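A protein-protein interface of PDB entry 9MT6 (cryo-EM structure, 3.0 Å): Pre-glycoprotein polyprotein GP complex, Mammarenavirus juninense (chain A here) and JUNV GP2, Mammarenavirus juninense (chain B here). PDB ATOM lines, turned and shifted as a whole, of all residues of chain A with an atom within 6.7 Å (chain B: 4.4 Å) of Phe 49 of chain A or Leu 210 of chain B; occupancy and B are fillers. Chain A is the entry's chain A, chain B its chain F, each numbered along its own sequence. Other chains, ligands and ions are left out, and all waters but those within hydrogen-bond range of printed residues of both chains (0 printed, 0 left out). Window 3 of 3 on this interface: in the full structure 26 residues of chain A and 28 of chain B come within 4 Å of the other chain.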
ATOM      1  N   PHE A  44     -12.555   9.845  13.982  1.00  0.00           N
ATOM      2  CA  PHE A  44     -13.048   8.894  14.971  1.00  0.00           C
ATOM      3  C   PHE A  44     -13.864   9.599  16.044  1.00  0.00           C
ATOM      4  O   PHE A  44     -14.925   9.110  16.451  1.00  0.00           O
ATOM      5  CB  PHE A  44     -11.880   8.134  15.596  1.00  0.00           C
ATOM      6  CG  PHE A  44     -11.150   7.247  14.631  1.00  0.00           C
ATOM      7  CD1 PHE A  44     -11.845   6.423  13.765  1.00  0.00           C
ATOM      8  CD2 PHE A  44      -9.766   7.229  14.597  1.00  0.00           C
ATOM      9  CE1 PHE A  44     -11.177   5.604  12.877  1.00  0.00           C
ATOM     10  CE2 PHE A  44      -9.090   6.410  13.713  1.00  0.00           C
ATOM     11  CZ  PHE A  44      -9.796   5.597  12.852  1.00  0.00           C
ATOM     12  N   GLN A  45     -13.386  10.754  16.512  1.00  0.00           N
ATOM     13  CA  GLN A  45     -14.139  11.524  17.495  1.00  0.00           C
ATOM     14  C   GLN A  45     -15.471  11.988  16.920  1.00  0.00           C
ATOM     15  O   GLN A  45     -16.491  11.991  17.620  1.00  0.00           O
ATOM     16  CB  GLN A  45     -13.309  12.716  17.967  1.00  0.00           C
ATOM     17  CG  GLN A  45     -13.956  13.536  19.066  1.00  0.00           C
ATOM     18  CD  GLN A  45     -13.069  14.670  19.541  1.00  0.00           C
ATOM     19  OE1 GLN A  45     -11.974  14.877  19.018  1.00  0.00           O
ATOM     20  NE2 GLN A  45     -13.538  15.410  20.539  1.00  0.00           N
ATOM     21  N   PHE A  46     -15.480  12.388  15.648  1.00  0.00           N
ATOM     22  CA  PHE A  46     -16.727  12.793  15.008  1.00  0.00           C
ATOM     23  C   PHE A  46     -17.715  11.636  14.937  1.00  0.00           C
ATOM     24  O   PHE A  46     -18.910  11.817  15.197  1.00  0.00           O
ATOM     25  CB  PHE A  46     -16.443  13.346  13.612  1.00  0.00           C
ATOM     26  CG  PHE A  46     -17.650  13.390  12.723  1.00  0.00           C
ATOM     27  CD1 PHE A  46     -18.625  14.353  12.904  1.00  0.00           C
ATOM     28  CD2 PHE A  46     -17.805  12.472  11.701  1.00  0.00           C
ATOM     29  CE1 PHE A  46     -19.734  14.396  12.088  1.00  0.00           C
ATOM     30  CE2 PHE A  46     -18.913  12.509  10.881  1.00  0.00           C
ATOM     31  CZ  PHE A  46     -19.879  13.472  11.073  1.00  0.00           C
ATOM     32  N   PHE A  47     -17.238  10.440  14.580  1.00  0.00           N
ATOM     33  CA  PHE A  47     -18.118   9.274  14.550  1.00  0.00           C
ATOM     34  C   PHE A  47     -18.649   8.942  15.939  1.00  0.00           C
ATOM     35  O   PHE A  47     -19.827   8.599  16.097  1.00  0.00           O
ATOM     36  CB  PHE A  47     -17.381   8.072  13.958  1.00  0.00           C
ATOM     37  CG  PHE A  47     -17.166   8.161  12.475  1.00  0.00           C
ATOM     38  CD1 PHE A  47     -17.884   9.064  11.713  1.00  0.00           C
ATOM     39  CD2 PHE A  47     -16.246   7.340  11.844  1.00  0.00           C
ATOM     40  CE1 PHE A  47     -17.690   9.147  10.348  1.00  0.00           C
ATOM     41  CE2 PHE A  47     -16.048   7.418  10.481  1.00  0.00           C
ATOM     42  CZ  PHE A  47     -16.771   8.323   9.733  1.00  0.00           C
ATOM     43  N   VAL A  48     -17.791   9.033  16.959  1.00  0.00           N
ATOM     44  CA  VAL A  48     -18.231   8.759  18.325  1.00  0.00           C
ATOM     45  C   VAL A  48     -19.300   9.756  18.751  1.00  0.00           C
ATOM     46  O   VAL A  48     -20.305   9.384  19.368  1.00  0.00           O
ATOM     47  CB  VAL A  48     -17.029   8.765  19.289  1.00  0.00           C
ATOM     48  CG1 VAL A  48     -17.501   8.649  20.729  1.00  0.00           C
ATOM     49  CG2 VAL A  48     -16.080   7.626  18.958  1.00  0.00           C
ATOM     50  N   PHE A  49     -19.105  11.037  18.428  1.00  0.00           N
ATOM     51  CA  PHE A  49     -20.111  12.039  18.767  1.00  0.00           C
ATOM     52  C   PHE A  49     -21.411  11.787  18.015  1.00  0.00           C
ATOM     53  O   PHE A  49     -22.501  11.950  18.573  1.00  0.00           O
ATOM     54  CB  PHE A  49     -19.587  13.446  18.472  1.00  0.00           C
ATOM     55  CG  PHE A  49     -20.664  14.499  18.417  1.00  0.00           C
ATOM     56  CD1 PHE A  49     -21.344  14.773  17.237  1.00  0.00           C
ATOM     57  CD2 PHE A  49     -21.000  15.213  19.554  1.00  0.00           C
ATOM     58  CE1 PHE A  49     -22.329  15.735  17.198  1.00  0.00           C
ATOM     59  CE2 PHE A  49     -21.985  16.177  19.520  1.00  0.00           C
ATOM     60  CZ  PHE A  49     -22.651  16.438  18.341  1.00  0.00           C
ATOM     61  N   LEU A  50     -21.314  11.411  16.739  1.00  0.00           N
ATOM     62  CA  LEU A  50     -22.513  11.139  15.955  1.00  0.00           C
ATOM     63  C   LEU A  50     -23.286   9.961  16.531  1.00  0.00           C
ATOM     64  O   LEU A  50     -24.522   9.961  16.539  1.00  0.00           O
ATOM     65  CB  LEU A  50     -22.138  10.885  14.497  1.00  0.00           C
ATOM     66  CG  LEU A  50     -23.286  10.660  13.515  1.00  0.00           C
ATOM     67  CD1 LEU A  50     -24.167  11.896  13.427  1.00  0.00           C
ATOM     68  CD2 LEU A  50     -22.747  10.287  12.144  1.00  0.00           C
ATOM     69  N   ALA A  51     -22.572   8.940  17.014  1.00  0.00           N
ATOM     70  CA  ALA A  51     -23.237   7.851  17.720  1.00  0.00           C
ATOM     71  C   ALA A  51     -23.885   8.346  19.008  1.00  0.00           C
ATOM     72  O   ALA A  51     -25.015   7.963  19.331  1.00  0.00           O
ATOM     73  CB  ALA A  51     -22.242   6.729  18.015  1.00  0.00           C
ATOM     74  N   LEU A  52     -23.188   9.201  19.752  1.00  0.00           N
ATOM     75  CA  LEU A  52     -23.713   9.767  20.995  1.00  0.00           C
ATOM     76  C   LEU A  52     -24.393  11.111  20.723  1.00  0.00           C
ATOM     77  O   LEU A  52     -24.041  12.151  21.277  1.00  0.00           O
ATOM     78  CB  LEU A  52     -22.597   9.906  22.023  1.00  0.00           C
ATOM     79  CG  LEU A  52     -21.838   8.628  22.386  1.00  0.00           C
ATOM     80  CD1 LEU A  52     -20.949   8.856  23.600  1.00  0.00           C
ATOM     81  CD2 LEU A  52     -22.800   7.475  22.631  1.00  0.00           C
ATOM     82  N   ALA A  53     -25.393  11.066  19.842  1.00  0.00           N
ATOM     83  CA  ALA A  53     -26.098  12.270  19.399  1.00  0.00           C
ATOM     84  C   ALA A  53     -27.106  12.677  20.470  1.00  0.00           C
ATOM     85  O   ALA A  53     -28.320  12.500  20.338  1.00  0.00           O
ATOM     86  CB  ALA A  53     -26.771  12.034  18.054  1.00  0.00           C
ATOM     87  N   GLY A  54     -26.581  13.238  21.557  1.00  0.00           N
ATOM     88  CA  GLY A  54     -27.402  13.701  22.656  1.00  0.00           C
ATOM     89  C   GLY A  54     -27.846  12.631  23.626  1.00  0.00           C
ATOM     90  O   GLY A  54     -28.506  12.957  24.619  1.00  0.00           O
ATOM     91  N   ARG A  55     -27.499  11.368  23.380  1.00  0.00           N
ATOM     92  CA  ARG A  55     -27.935  10.272  24.232  1.00  0.00           C
ATOM     93  C   ARG A  55     -27.178  10.199  25.551  1.00  0.00           C
ATOM     94  O   ARG A  55     -27.636   9.511  26.469  1.00  0.00           O
ATOM     95  CB  ARG A  55     -27.790   8.943  23.488  1.00  0.00           C
ATOM     96  CG  ARG A  55     -28.491   8.910  22.143  1.00  0.00           C
ATOM     97  CD  ARG A  55     -27.719   8.065  21.143  1.00  0.00           C
ATOM     98  NE  ARG A  55     -27.639   6.669  21.555  1.00  0.00           N
ATOM     99  CZ  ARG A  55     -28.578   5.764  21.319  1.00  0.00           C
ATOM    100  NH1 ARG A  55     -29.688   6.072  20.669  1.00  0.00           N
ATOM    101  NH2 ARG A  55     -28.398   4.516  21.743  1.00  0.00           N
ATOM    102  N   SER A  56     -26.043  10.882  25.672  1.00  0.00           N
ATOM    103  CA  SER A  56     -25.268  10.869  26.905  1.00  0.00           C
ATOM    104  C   SER A  56     -24.511  12.184  27.010  1.00  0.00           C
ATOM    105  O   SER A  56     -24.520  13.004  26.090  1.00  0.00           O
ATOM    106  CB  SER A  56     -24.306   9.679  26.957  1.00  0.00           C
ATOM    107  OG  SER A  56     -24.979   8.459  26.695  1.00  0.00           O
ATOM    108  N   THR B 195     -16.101  17.832  15.246  1.00  0.00           N
ATOM    109  CA  THR B 195     -16.440  16.746  16.156  1.00  0.00           C
ATOM    110  C   THR B 195     -17.762  16.980  16.874  1.00  0.00           C
ATOM    111  O   THR B 195     -18.696  16.189  16.722  1.00  0.00           O
ATOM    112  CB  THR B 195     -15.314  16.557  17.181  1.00  0.00           C
ATOM    113  OG1 THR B 195     -15.164  17.756  17.954  1.00  0.00           O
ATOM    114  CG2 THR B 195     -14.001  16.249  16.479  1.00  0.00           C
ATOM    115  N   HIS B 196     -17.873  18.056  17.643  1.00  0.00           N
ATOM    116  CA  HIS B 196     -19.084  18.359  18.387  1.00  0.00           C
ATOM    117  C   HIS B 196     -20.009  19.237  17.554  1.00  0.00           C
ATOM    118  O   HIS B 196     -19.792  19.460  16.361  1.00  0.00           O
ATOM    119  CB  HIS B 196     -18.741  19.034  19.718  1.00  0.00           C
ATOM    120  CG  HIS B 196     -17.741  20.139  19.592  1.00  0.00           C
ATOM    121  ND1 HIS B 196     -17.932  21.225  18.768  1.00  0.00           N
ATOM    122  CD2 HIS B 196     -16.539  20.324  20.185  1.00  0.00           C
ATOM    123  CE1 HIS B 196     -16.893  22.034  18.861  1.00  0.00           C
ATOM    124  NE2 HIS B 196     -16.032  21.508  19.712  1.00  0.00           N
ATOM    125  N   ARG B 197     -21.052  19.742  18.201  1.00  0.00           N
ATOM    126  CA  ARG B 197     -22.091  20.518  17.530  1.00  0.00           C
ATOM    127  C   ARG B 197     -22.404  21.727  18.406  1.00  0.00           C
ATOM    128  O   ARG B 197     -23.076  21.599  19.433  1.00  0.00           O
ATOM    129  CB  ARG B 197     -23.321  19.651  17.284  1.00  0.00           C
ATOM    130  CG  ARG B 197     -24.399  20.262  16.412  1.00  0.00           C
ATOM    131  CD  ARG B 197     -25.495  19.238  16.173  1.00  0.00           C
ATOM    132  NE  ARG B 197     -26.631  19.785  15.440  1.00  0.00           N
ATOM    133  CZ  ARG B 197     -26.708  19.850  14.118  1.00  0.00           C
ATOM    134  NH1 ARG B 197     -25.737  19.390  13.347  1.00  0.00           N
ATOM    135  NH2 ARG B 197     -27.789  20.382  13.556  1.00  0.00           N
ATOM    136  N   ILE B 199     -23.544  26.087  18.661  1.00  0.00           N
ATOM    137  CA  ILE B 199     -24.662  26.918  18.229  1.00  0.00           C
ATOM    138  C   ILE B 199     -24.129  28.312  17.929  1.00  0.00           C
ATOM    139  O   ILE B 199     -23.223  28.797  18.617  1.00  0.00           O
ATOM    140  CB  ILE B 199     -25.780  26.969  19.295  1.00  0.00           C
ATOM    141  CG1 ILE B 199     -26.372  25.577  19.526  1.00  0.00           C
ATOM    142  CG2 ILE B 199     -26.884  27.933  18.888  1.00  0.00           C
ATOM    143  CD1 ILE B 199     -27.292  25.498  20.725  1.00  0.00           C
ATOM    144  N   HIS B 208     -21.581  18.166  26.710  1.00  0.00           N
ATOM    145  CA  HIS B 208     -23.025  18.025  26.562  1.00  0.00           C
ATOM    146  C   HIS B 208     -23.386  17.926  25.084  1.00  0.00           C
ATOM    147  O   HIS B 208     -23.285  18.913  24.350  1.00  0.00           O
ATOM    148  CB  HIS B 208     -23.754  19.194  27.230  1.00  0.00           C
ATOM    149  CG  HIS B 208     -25.234  19.004  27.347  1.00  0.00           C
ATOM    150  ND1 HIS B 208     -25.799  17.944  28.024  1.00  0.00           N
ATOM    151  CD2 HIS B 208     -26.265  19.758  26.898  1.00  0.00           C
ATOM    152  CE1 HIS B 208     -27.115  18.044  27.969  1.00  0.00           C
ATOM    153  NE2 HIS B 208     -27.424  19.137  27.296  1.00  0.00           N
ATOM    154  N   ARG B 209     -23.820  16.750  24.643  1.00  0.00           N
ATOM    155  CA  ARG B 209     -24.049  16.515  23.226  1.00  0.00           C
ATOM    156  C   ARG B 209     -25.371  17.130  22.780  1.00  0.00           C
ATOM    157  O   ARG B 209     -26.288  17.355  23.574  1.00  0.00           O
ATOM    158  CB  ARG B 209     -24.037  15.019  22.913  1.00  0.00           C
ATOM    159  CG  ARG B 209     -22.951  14.240  23.638  1.00  0.00           C
ATOM    160  CD  ARG B 209     -21.566  14.746  23.278  1.00  0.00           C
ATOM    161  NE  ARG B 209     -20.623  14.586  24.379  1.00  0.00           N
ATOM    162  CZ  ARG B 209     -20.088  13.430  24.748  1.00  0.00           C
ATOM    163  NH1 ARG B 209     -20.374  12.302  24.120  1.00  0.00           N
ATOM    164  NH2 ARG B 209     -19.240  13.408  25.772  1.00  0.00           N
ATOM    165  N   LEU B 210     -25.459  17.398  21.477  1.00  0.00           N
ATOM    166  CA  LEU B 210     -26.625  18.026  20.876  1.00  0.00           C
ATOM    167  C   LEU B 210     -27.142  17.160  19.739  1.00  0.00           C
ATOM    168  O   LEU B 210     -26.378  16.445  19.084  1.00  0.00           O
ATOM    169  CB  LEU B 210     -26.295  19.429  20.354  1.00  0.00           C
ATOM    170  CG  LEU B 210     -25.925  20.482  21.399  1.00  0.00           C
ATOM    171  CD1 LEU B 210     -25.939  21.870  20.784  1.00  0.00           C
ATOM    172  CD2 LEU B 210     -26.863  20.416  22.594  1.00  0.00           C
ATOM    173  N   ASN B 211     -28.450  17.228  19.508  1.00  0.00           N
ATOM    174  CA  ASN B 211     -29.088  16.449  18.459  1.00  0.00           C
ATOM    175  C   ASN B 211     -29.065  17.241  17.154  1.00  0.00           C
ATOM    176  O   ASN B 211     -28.382  18.262  17.034  1.00  0.00           O
ATOM    177  CB  ASN B 211     -30.507  16.057  18.873  1.00  0.00           C
ATOM    178  CG  ASN B 211     -31.420  17.257  19.064  1.00  0.00           C
ATOM    179  OD1 ASN B 211     -30.985  18.406  18.998  1.00  0.00           O
ATOM    180  ND2 ASN B 211     -32.696  16.992  19.309  1.00  0.00           N
ATOM    181  N   GLY B 214     -29.909  20.660  17.868  1.00  0.00           N
ATOM    182  CA  GLY B 214     -29.163  21.261  18.961  1.00  0.00           C
ATOM    183  C   GLY B 214     -29.811  21.100  20.320  1.00  0.00           C
ATOM    184  O   GLY B 214     -29.864  22.062  21.096  1.00  0.00           O
ATOM    185  N   GLY B 215     -30.304  19.898  20.631  1.00  0.00           N
ATOM    186  CA  GLY B 215     -30.949  19.632  21.898  1.00  0.00           C
ATOM    187  C   GLY B 215     -30.418  18.363  22.542  1.00  0.00           C
ATOM    188  O   GLY B 215     -29.656  17.605  21.940  1.00  0.00           O
ATOM    189  N   TYR B 221     -29.038  22.193  27.274  1.00  0.00           N
ATOM    190  CA  TYR B 221     -29.246  22.871  25.997  1.00  0.00           C
ATOM    191  C   TYR B 221     -30.328  22.106  25.249  1.00  0.00           C
ATOM    192  O   TYR B 221     -30.031  21.296  24.359  1.00  0.00           O
ATOM    193  CB  TYR B 221     -27.951  22.957  25.188  1.00  0.00           C
ATOM    194  CG  TYR B 221     -26.885  23.807  25.839  1.00  0.00           C
ATOM    195  CD1 TYR B 221     -26.838  25.178  25.626  1.00  0.00           C
ATOM    196  CD2 TYR B 221     -25.923  23.240  26.665  1.00  0.00           C
ATOM    197  CE1 TYR B 221     -25.868  25.962  26.220  1.00  0.00           C
ATOM    198  CE2 TYR B 221     -24.947  24.016  27.261  1.00  0.00           C
ATOM    199  CZ  TYR B 221     -24.923  25.375  27.035  1.00  0.00           C
ATOM    200  OH  TYR B 221     -23.955  26.153  27.626  1.00  0.00           O
ATOM    201  N   TRP B 230     -20.634  23.757  13.338  1.00  0.00           N
ATOM    202  CA  TRP B 230     -19.765  22.583  13.361  1.00  0.00           C
ATOM    203  C   TRP B 230     -18.324  23.064  13.450  1.00  0.00           C
ATOM    204  O   TRP B 230     -17.626  23.181  12.442  1.00  0.00           O
ATOM    205  CB  TRP B 230     -19.985  21.731  12.118  1.00  0.00           C
ATOM    206  CG  TRP B 230     -21.179  20.838  12.177  1.00  0.00           C
ATOM    207  CD1 TRP B 230     -22.411  21.081  11.648  1.00  0.00           C
ATOM    208  CD2 TRP B 230     -21.244  19.534  12.764  1.00  0.00           C
ATOM    209  NE1 TRP B 230     -23.246  20.017  11.887  1.00  0.00           N
ATOM    210  CE2 TRP B 230     -22.551  19.054  12.569  1.00  0.00           C
ATOM    211  CE3 TRP B 230     -20.324  18.730  13.440  1.00  0.00           C
ATOM    212  CZ2 TRP B 230     -22.964  17.806  13.029  1.00  0.00           C
ATOM    213  CZ3 TRP B 230     -20.735  17.492  13.897  1.00  0.00           C
ATOM    214  CH2 TRP B 230     -22.043  17.042  13.689  1.00  0.00           C
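O of Asn 211 of chain B lies within hydrogen-bond range of NE of Arg 197 of chain B (2.8 Å).
Among the printed residues, pairs that only touch across the chains: Phe 49 of chain A with Thr 195 of chain B (3.0 Å), Ser 56 of chain A with Arg 209 of chain B (3.2 Å), Leu 52 of chain A with Arg 209 of chain B (3.3 Å), Gly 54 of chain A with Arg 209 of chain B (3.4 Å), Phe 49 of chain A with Arg 197 of chain B (3.4 Å), Gln 45 of chain A with Thr 195 of chain B (3.5 Å), Phe 46 of chain A with Trp 230 of chain B (3.7 Å), Phe 49 of chain A with Trp 230 of chain B (3.8 Å), Phe 49 of chain A with Arg 209 of chain B (3.8 Å), Phe 49 of chain A with Leu 210 of chain B (3.8 Å) and Phe 49 of chain A with His 196 of chain B (3.8 Å).
Of the printed residues of chain A, Leu 210 of chain B touches Phe 49 (3.8 Å). Printed residues of chain A within 4 Å of His 196 of chain B: Phe 49 (3.8 Å). Printed residues of chain B within 4 Å of Gln 45 of chain A: Thr 195. Printed residues of chain A within 4 Å of Thr 195 of chain B: Gln 45 and Phe 49. Printed residues of chain A within 4 Å of Arg 197 of chain B: Phe 49 (3.4 Å). Of the printed residues of chain B, Leu 52 of chain A touches Arg 209. Gly 214 of chain B touches none of the printed residues of chain A. Asn 211 of chain B touches none of the printed residues of chain A. The nearest printed residue of chain A that does not touch Leu 210 of chain B is Gly 54 of chain A (4.1 Å).
Hydrophobic or aromatic side chains of chain B that line the printed part of chain A: Trp 230. Along chain A the printed residues that touch a printed residue of chain B span positions 45 to 56. Among the printed residues, no Asp or Glu carboxylate lies within 4 Å of a Lys or Arg side-chain nitrogen of the other chain.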
